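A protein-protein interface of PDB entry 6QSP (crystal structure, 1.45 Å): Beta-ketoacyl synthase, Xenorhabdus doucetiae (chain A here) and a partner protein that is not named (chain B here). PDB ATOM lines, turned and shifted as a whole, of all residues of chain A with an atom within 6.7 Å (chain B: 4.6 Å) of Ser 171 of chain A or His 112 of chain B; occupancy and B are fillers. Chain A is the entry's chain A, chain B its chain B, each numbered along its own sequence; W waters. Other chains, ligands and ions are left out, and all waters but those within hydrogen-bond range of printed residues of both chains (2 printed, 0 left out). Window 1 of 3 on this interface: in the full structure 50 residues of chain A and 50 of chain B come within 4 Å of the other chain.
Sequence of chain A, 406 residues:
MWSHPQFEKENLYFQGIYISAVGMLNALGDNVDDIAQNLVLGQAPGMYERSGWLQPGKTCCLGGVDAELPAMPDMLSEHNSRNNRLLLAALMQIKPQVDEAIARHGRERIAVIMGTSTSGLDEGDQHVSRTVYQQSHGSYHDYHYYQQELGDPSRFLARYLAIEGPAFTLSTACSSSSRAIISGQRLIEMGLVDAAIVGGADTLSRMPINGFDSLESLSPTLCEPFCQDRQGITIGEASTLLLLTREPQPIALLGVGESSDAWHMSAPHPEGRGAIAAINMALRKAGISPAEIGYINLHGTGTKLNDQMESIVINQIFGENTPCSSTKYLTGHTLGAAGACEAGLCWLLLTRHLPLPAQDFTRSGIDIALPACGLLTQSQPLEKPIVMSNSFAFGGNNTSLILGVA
The backbone NH (N) of Ser 171 of chain A sits at hydrogen-bond distance from the backbone carbonyl oxygen (O) of Ser 131 of chain B, at 2.9 Å.
The backbone carbonyl oxygen of Ser 171 of chain A is in hydrogen-bond range of the backbone NH of Asn 113 of chain B, at 3.5 Å.
O of Thr 169 of chain A is in hydrogen-bond range of N of Ser 133 of chain B (2.9 Å).
O of Ser 81 of chain B is in hydrogen-bond range of NE2 of His 112 of chain B, 2.9 Å away.
The backbone NH (N) of Val 132 of chain B is in hydrogen-bond range of the backbone carbonyl oxygen (O) of Tyr 79 of chain B (2.9 Å).
The backbone carbonyl oxygen of Ser 81 of chain B is in hydrogen-bond range of the side-chain hydroxyl of Ser 133 of chain B.
OG1 of Thr 172 of chain A sits at hydrogen-bond distance from OG of Ser 175 of chain A, at 2.8 Å.
The backbone NH (N) of Ser 81 of chain B lies within hydrogen-bond range of the backbone carbonyl oxygen (O) of Val 132 of chain B, at 3.0 Å.
The backbone carbonyl oxygen of Thr 116 of chain A sits at hydrogen-bond distance from the side-chain hydroxyl of Ser 171 of chain A.
Among the printed residues, pairs that only touch across the chains: Ser 171 of chain A with His 112 of chain B (3.4 Å), Thr 169 of chain A with Val 132 of chain B (3.4 Å), Leu 170 of chain A with Ser 131 of chain B (3.5 Å), Thr 172 of chain A with Asn 113 of chain B (3.6 Å), Thr 172 of chain A with Ser 131 of chain B (3.6 Å), Ala 173 of chain A with Asn 113 of chain B (3.7 Å), Leu 150 of chain A with His 112 of chain B (3.7 Å) and Leu 150 of chain A with Ser 133 of chain B (3.9 Å).
Ser 171 of chain A touches just these residues of chain B: His 112 (3.4 Å), Asn 113 (3.5 Å) and Ser 131 (2.9 Å).
Of the printed residues of chain B, Thr 172 of chain A touches Asn 113 and Ser 131.
Ser 176 of chain A touches none of the printed residues of chain B.
Tyr 79 of chain B touches none of the printed residues of chain A.
Of chain A, only Leu 150 and Ser 171 come within 4 Å of His 112 of chain B.
Printed residues of chain A within 4 Å of Asn 113 of chain B: Ser 171, Thr 172 and Ala 173.
Printed residues of chain A within 4 Å of Ser 131 of chain B: Leu 170, Ser 171 and Thr 172.
Of the printed residues of chain A, Val 132 of chain B touches Thr 169.
Of the printed residues of chain A, Ser 133 of chain B touches Leu 150 (3.9 Å) and Thr 169 (2.9 Å).
The nearest printed residue of chain B that does not touch Ser 171 of chain A is Val 132 of chain B (4.8 Å).
The nearest residue of chain A that does not touch His 112 of chain B is Thr 172 of chain A (5.5 Å).
Of the 13 printed residues of chain B, 5 touch a printed residue of chain A.
Printed residues of chain B that touch a printed residue of chain A: His 112, Asn 113, Ser 131, Val 132 and Ser 133.
Along chain B the printed residues that touch a printed residue of chain A span positions 112 to 133.
Of the 13 printed residues of chain A, 6 touch a printed residue of chain B.
Hydrophobic or aromatic side chains of chain A that line the printed part of chain B: Leu 150, Leu 170 and Ala 173.
Among the printed residues, 11 pairs touch across the chains.
Water W2 lies within hydrogen-bond range of OG of Ser 171 of chain A (2.7 Å), N of His 112 of chain B (3.2 Å) and N of Ala 173 of chain A (3.3 Å).
Water W1 bridges the backbone NH of His 112 of chain B (3.4 Å) and the backbone carbonyl oxygen of Ser 117 of chain A (3.4 Å).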
ATOM      1  N   MET A 114       0.869 -28.109   8.840  1.00  0.00           N
ATOM      2  CA  MET A 114       2.024 -27.926   7.944  1.00  0.00           C
ATOM      3  C   MET A 114       1.547 -27.345   6.612  1.00  0.00           C
ATOM      4  O   MET A 114       0.337 -27.350   6.329  1.00  0.00           O
ATOM      5  CB  MET A 114       2.727 -29.261   7.713  1.00  0.00           C
ATOM      6  CG  MET A 114       3.406 -29.803   8.958  1.00  0.00           C
ATOM      7  SD  MET A 114       4.777 -28.749   9.520  1.00  0.00           S
ATOM      8  CE  MET A 114       4.127 -28.137  11.073  1.00  0.00           C
ATOM      9  N   GLY A 115       2.504 -26.904   5.813  1.00  0.00           N
ATOM     10  CA  GLY A 115       2.297 -26.544   4.403  1.00  0.00           C
ATOM     11  C   GLY A 115       3.425 -27.122   3.571  1.00  0.00           C
ATOM     12  O   GLY A 115       4.581 -27.126   4.029  1.00  0.00           O
ATOM     13  N   THR A 116       3.106 -27.616   2.388  1.00  0.00           N
ATOM     14  CA  THR A 116       4.125 -28.091   1.432  1.00  0.00           C
ATOM     15  C   THR A 116       3.544 -28.054   0.030  1.00  0.00           C
ATOM     16  O   THR A 116       2.326 -28.263  -0.133  1.00  0.00           O
ATOM     17  CB  THR A 116       4.651 -29.497   1.769  1.00  0.00           C
ATOM     18  OG1 THR A 116       5.837 -29.764   1.012  1.00  0.00           O
ATOM     19  CG2 THR A 116       3.640 -30.573   1.471  1.00  0.00           C
ATOM     20  N   SER A 117       4.423 -27.839  -0.942  1.00  0.00           N
ATOM     21  CA  SER A 117       4.115 -28.029  -2.376  1.00  0.00           C
ATOM     22  C   SER A 117       4.839 -29.272  -2.903  1.00  0.00           C
ATOM     23  O   SER A 117       4.541 -29.650  -4.037  1.00  0.00           O
ATOM     24  CB  SER A 117       4.434 -26.789  -3.176  1.00  0.00           C
ATOM     25  OG  SER A 117       5.804 -26.749  -3.546  1.00  0.00           O
ATOM     26  N   THR A 118       5.742 -29.892  -2.131  1.00  0.00           N
ATOM     27  CA  THR A 118       6.516 -31.071  -2.618  1.00  0.00           C
ATOM     28  C   THR A 118       6.240 -32.340  -1.815  1.00  0.00           C
ATOM     29  O   THR A 118       6.210 -33.414  -2.426  1.00  0.00           O
ATOM     30  CB  THR A 118       8.040 -30.849  -2.629  1.00  0.00           C
ATOM     31  OG1 THR A 118       8.575 -30.664  -1.314  1.00  0.00           O
ATOM     32  CG2 THR A 118       8.434 -29.674  -3.490  1.00  0.00           C
ATOM     33  N   LEU A 150       1.023 -35.465  -0.042  1.00  0.00           N
ATOM     34  CA  LEU A 150       1.098 -34.061   0.429  1.00  0.00           C
ATOM     35  C   LEU A 150       0.678 -33.934   1.898  1.00  0.00           C
ATOM     36  O   LEU A 150       1.095 -32.960   2.520  1.00  0.00           O
ATOM     37  CB  LEU A 150       0.296 -33.144  -0.496  1.00  0.00           C
ATOM     38  CG  LEU A 150       0.919 -32.944  -1.880  1.00  0.00           C
ATOM     39  CD1 LEU A 150      -0.050 -32.261  -2.823  1.00  0.00           C
ATOM     40  CD2 LEU A 150       2.220 -32.160  -1.799  1.00  0.00           C
ATOM     41  N   THR A 169      -2.165 -30.765   6.348  1.00  0.00           N
ATOM     42  CA  THR A 169      -1.212 -29.988   5.528  1.00  0.00           C
ATOM     43  C   THR A 169      -1.982 -29.144   4.506  1.00  0.00           C
ATOM     44  O   THR A 169      -2.856 -29.676   3.798  1.00  0.00           O
ATOM     45  CB  THR A 169      -0.186 -30.927   4.883  1.00  0.00           C
ATOM     46  OG1 THR A 169       0.473 -31.688   5.908  1.00  0.00           O
ATOM     47  CG2 THR A 169       0.853 -30.166   4.085  1.00  0.00           C
ATOM     48  N   LEU A 170      -1.666 -27.859   4.452  1.00  0.00           N
ATOM     49  CA  LEU A 170      -2.142 -26.942   3.390  1.00  0.00           C
ATOM     50  C   LEU A 170      -1.264 -27.181   2.162  1.00  0.00           C
ATOM     51  O   LEU A 170      -0.032 -27.251   2.303  1.00  0.00           O
ATOM     52  CB  LEU A 170      -2.006 -25.485   3.836  1.00  0.00           C
ATOM     53  CG  LEU A 170      -3.057 -24.920   4.783  1.00  0.00           C
ATOM     54  CD1 LEU A 170      -4.389 -24.824   4.078  1.00  0.00           C
ATOM     55  CD2 LEU A 170      -3.168 -25.720   6.056  1.00  0.00           C
ATOM     56  N   SER A 171      -1.858 -27.263   0.983  1.00  0.00           N
ATOM     57  CA  SER A 171      -1.074 -27.317  -0.276  1.00  0.00           C
ATOM     58  C   SER A 171      -1.688 -26.323  -1.262  1.00  0.00           C
ATOM     59  O   SER A 171      -2.511 -26.720  -2.096  1.00  0.00           O
ATOM     60  CB  SER A 171      -0.950 -28.720  -0.800  1.00  0.00           C
ATOM     61  OG  SER A 171       0.129 -28.794  -1.726  1.00  0.00           O
ATOM     62  N   THR A 172      -1.363 -25.050  -1.052  1.00  0.00           N
ATOM     63  CA  THR A 172      -1.766 -23.904  -1.901  1.00  0.00           C
ATOM     64  C   THR A 172      -0.509 -23.324  -2.541  1.00  0.00           C
ATOM     65  O   THR A 172      -0.324 -22.109  -2.502  1.00  0.00           O
ATOM     66  CB  THR A 172      -2.589 -22.894  -1.087  1.00  0.00           C
ATOM     67  OG1 THR A 172      -1.828 -22.421   0.033  1.00  0.00           O
ATOM     68  CG2 THR A 172      -3.894 -23.505  -0.618  1.00  0.00           C
ATOM     69  N   ALA A 173       0.315 -24.171  -3.153  1.00  0.00           N
ATOM     70  CA  ALA A 173       1.521 -23.710  -3.876  1.00  0.00           C
ATOM     71  C   ALA A 173       2.336 -22.811  -2.929  1.00  0.00           C
ATOM     72  O   ALA A 173       2.536 -23.238  -1.769  1.00  0.00           O
ATOM     73  CB  ALA A 173       1.112 -23.040  -5.171  1.00  0.00           C
ATOM     74  N   SER A 175       1.895 -20.301  -1.075  1.00  0.00           N
ATOM     75  CA  SER A 175       1.303 -19.754   0.180  1.00  0.00           C
ATOM     76  C   SER A 175       1.030 -20.855   1.213  1.00  0.00           C
ATOM     77  O   SER A 175       0.468 -20.541   2.284  1.00  0.00           O
ATOM     78  CB  SER A 175       0.060 -18.952  -0.102  1.00  0.00           C
ATOM     79  OG  SER A 175      -0.970 -19.796  -0.570  1.00  0.00           O
ATOM     80  N   SER A 176       1.426 -22.095   0.934  1.00  0.00           N
ATOM     81  CA  SER A 176       1.063 -23.266   1.771  1.00  0.00           C
ATOM     82  C   SER A 176       1.430 -23.020   3.238  1.00  0.00           C
ATOM     83  O   SER A 176       0.575 -23.200   4.119  1.00  0.00           O
ATOM     84  CB  SER A 176       1.724 -24.521   1.257  1.00  0.00           C
ATOM     85  OG  SER A 176       1.237 -24.868  -0.031  1.00  0.00           O
ATOM     86  N   TYR B  79     -11.099 -27.008  -0.654  1.00  0.00           N
ATOM     87  CA  TYR B  79     -11.011 -28.306  -1.363  1.00  0.00           C
ATOM     88  C   TYR B  79     -10.075 -29.212  -0.555  1.00  0.00           C
ATOM     89  O   TYR B  79      -9.095 -28.731   0.056  1.00  0.00           O
ATOM     90  CB  TYR B  79     -10.562 -28.118  -2.819  1.00  0.00           C
ATOM     91  CG  TYR B  79     -11.675 -27.825  -3.804  1.00  0.00           C
ATOM     92  CD1 TYR B  79     -12.648 -26.886  -3.516  1.00  0.00           C
ATOM     93  CD2 TYR B  79     -11.777 -28.496  -5.014  1.00  0.00           C
ATOM     94  CE1 TYR B  79     -13.691 -26.624  -4.392  1.00  0.00           C
ATOM     95  CE2 TYR B  79     -12.819 -28.249  -5.906  1.00  0.00           C
ATOM     96  CZ  TYR B  79     -13.789 -27.310  -5.589  1.00  0.00           C
ATOM     97  OH  TYR B  79     -14.844 -27.074  -6.434  1.00  0.00           O
ATOM     98  N   THR B  80     -10.394 -30.502  -0.520  1.00  0.00           N
ATOM     99  CA  THR B  80      -9.584 -31.529   0.163  1.00  0.00           C
ATOM    100  C   THR B  80      -9.325 -32.668  -0.814  1.00  0.00           C
ATOM    101  O   THR B  80     -10.231 -33.037  -1.592  1.00  0.00           O
ATOM    102  CB  THR B  80     -10.238 -32.052   1.452  1.00  0.00           C
ATOM    103  OG1 THR B  80     -11.473 -32.721   1.198  1.00  0.00           O
ATOM    104  CG2 THR B  80     -10.523 -30.961   2.448  1.00  0.00           C
ATOM    105  N   SER B  81      -8.121 -33.226  -0.757  1.00  0.00           N
ATOM    106  CA  SER B  81      -7.788 -34.424  -1.559  1.00  0.00           C
ATOM    107  C   SER B  81      -6.575 -35.093  -0.941  1.00  0.00           C
ATOM    108  O   SER B  81      -5.580 -34.402  -0.650  1.00  0.00           O
ATOM    109  CB  SER B  81      -7.543 -34.057  -3.006  1.00  0.00           C
ATOM    110  OG  SER B  81      -7.146 -35.193  -3.769  1.00  0.00           O
ATOM    111  N   GLY B  84      -4.318 -35.703  -4.440  1.00  0.00           N
ATOM    112  CA  GLY B  84      -4.163 -34.503  -5.277  1.00  0.00           C
ATOM    113  C   GLY B  84      -4.064 -34.849  -6.750  1.00  0.00           C
ATOM    114  O   GLY B  84      -4.763 -35.777  -7.207  1.00  0.00           O
ATOM    115  N   SER B 110      -0.710 -29.035 -11.821  1.00  0.00           N
ATOM    116  CA  SER B 110      -0.299 -30.150 -10.923  1.00  0.00           C
ATOM    117  C   SER B 110      -0.339 -29.708  -9.459  1.00  0.00           C
ATOM    118  O   SER B 110      -0.308 -30.599  -8.581  1.00  0.00           O
ATOM    119  CB  SER B 110       1.059 -30.701 -11.272  1.00  0.00           C
ATOM    120  OG  SER B 110       2.097 -29.807 -10.878  1.00  0.00           O
ATOM    121  N   VAL B 111      -0.404 -28.400  -9.189  1.00  0.00           N
ATOM    122  CA  VAL B 111      -0.508 -27.909  -7.783  1.00  0.00           C
ATOM    123  C   VAL B 111      -1.834 -28.412  -7.196  1.00  0.00           C
ATOM    124  O   VAL B 111      -2.853 -28.492  -7.914  1.00  0.00           O
ATOM    125  CB  VAL B 111      -0.348 -26.382  -7.647  1.00  0.00           C
ATOM    126  CG1 VAL B 111       1.015 -25.918  -8.133  1.00  0.00           C
ATOM    127  CG2 VAL B 111      -1.461 -25.597  -8.318  1.00  0.00           C
ATOM    128  N   HIS B 112      -1.818 -28.777  -5.918  1.00  0.00           N
ATOM    129  CA  HIS B 112      -3.004 -29.367  -5.254  1.00  0.00           C
ATOM    130  C   HIS B 112      -4.195 -28.409  -5.376  1.00  0.00           C
ATOM    131  O   HIS B 112      -5.329 -28.886  -5.588  1.00  0.00           O
ATOM    132  CB  HIS B 112      -2.642 -29.688  -3.801  1.00  0.00           C
ATOM    133  CG  HIS B 112      -3.668 -30.445  -3.030  1.00  0.00           C
ATOM    134  ND1 HIS B 112      -4.778 -29.840  -2.485  1.00  0.00           N
ATOM    135  CD2 HIS B 112      -3.718 -31.747  -2.655  1.00  0.00           C
ATOM    136  CE1 HIS B 112      -5.466 -30.733  -1.811  1.00  0.00           C
ATOM    137  NE2 HIS B 112      -4.841 -31.915  -1.891  1.00  0.00           N
ATOM    138  N   ASN B 113      -3.942 -27.103  -5.245  1.00  0.00           N
ATOM    139  CA  ASN B 113      -5.020 -26.080  -5.261  1.00  0.00           C
ATOM    140  C   ASN B 113      -5.414 -25.723  -6.698  1.00  0.00           C
ATOM    141  O   ASN B 113      -6.137 -24.744  -6.852  1.00  0.00           O
ATOM    142  CB  ASN B 113      -4.673 -24.830  -4.442  1.00  0.00           C
ATOM    143  CG  ASN B 113      -3.521 -24.022  -4.988  1.00  0.00           C
ATOM    144  OD1 ASN B 113      -2.522 -24.592  -5.419  1.00  0.00           O
ATOM    145  ND2 ASN B 113      -3.631 -22.697  -4.919  1.00  0.00           N
ATOM    146  N   SER B 114      -5.025 -26.476  -7.733  1.00  0.00           N
ATOM    147  CA  SER B 114      -5.471 -26.094  -9.100  1.00  0.00           C
ATOM    148  C   SER B 114      -6.996 -26.229  -9.214  1.00  0.00           C
ATOM    149  O   SER B 114      -7.610 -25.402  -9.901  1.00  0.00           O
ATOM    150  CB  SER B 114      -4.765 -26.862 -10.171  1.00  0.00           C
ATOM    151  OG  SER B 114      -5.197 -28.194 -10.175  1.00  0.00           O
ATOM    152  N   SER B 115      -7.614 -27.198  -8.549  1.00  0.00           N
ATOM    153  CA  SER B 115      -9.090 -27.379  -8.593  1.00  0.00           C
ATOM    154  C   SER B 115      -9.783 -26.144  -8.006  1.00  0.00           C
ATOM    155  O   SER B 115     -10.624 -25.533  -8.700  1.00  0.00           O
ATOM    156  CB  SER B 115      -9.532 -28.622  -7.880  1.00  0.00           C
ATOM    157  OG  SER B 115      -9.112 -29.810  -8.537  1.00  0.00           O
ATOM    158  N   SER B 131      -6.784 -25.361   0.309  1.00  0.00           N
ATOM    159  CA  SER B 131      -6.663 -26.706  -0.289  1.00  0.00           C
ATOM    160  C   SER B 131      -5.864 -27.548   0.705  1.00  0.00           C
ATOM    161  O   SER B 131      -4.774 -27.100   1.101  1.00  0.00           O
ATOM    162  CB  SER B 131      -6.055 -26.606  -1.665  1.00  0.00           C
ATOM    163  OG  SER B 131      -6.484 -27.662  -2.501  1.00  0.00           O
ATOM    164  N   VAL B 132      -6.448 -28.666   1.140  1.00  0.00           N
ATOM    165  CA  VAL B 132      -5.936 -29.474   2.282  1.00  0.00           C
ATOM    166  C   VAL B 132      -5.654 -30.906   1.836  1.00  0.00           C
ATOM    167  O   VAL B 132      -6.456 -31.486   1.112  1.00  0.00           O
ATOM    168  CB  VAL B 132      -6.930 -29.450   3.459  1.00  0.00           C
ATOM    169  CG1 VAL B 132      -6.497 -30.354   4.588  1.00  0.00           C
ATOM    170  CG2 VAL B 132      -7.155 -28.041   3.969  1.00  0.00           C
ATOM    171  N   SER B 133      -4.571 -31.471   2.363  1.00  0.00           N
ATOM    172  CA  SER B 133      -4.247 -32.905   2.240  1.00  0.00           C
ATOM    173  C   SER B 133      -3.869 -33.416   3.631  1.00  0.00           C
ATOM    174  O   SER B 133      -3.091 -32.732   4.337  1.00  0.00           O
ATOM    175  CB  SER B 133      -3.155 -33.115   1.225  1.00  0.00           C
ATOM    176  OG  SER B 133      -3.118 -34.461   0.805  1.00  0.00           O
HETATM  177  O   HOH W   1       1.527 -29.011  -5.520  1.00  0.00           O
HETATM  178  O   HOH W   2       0.350 -27.317  -4.022  1.00  0.00           O
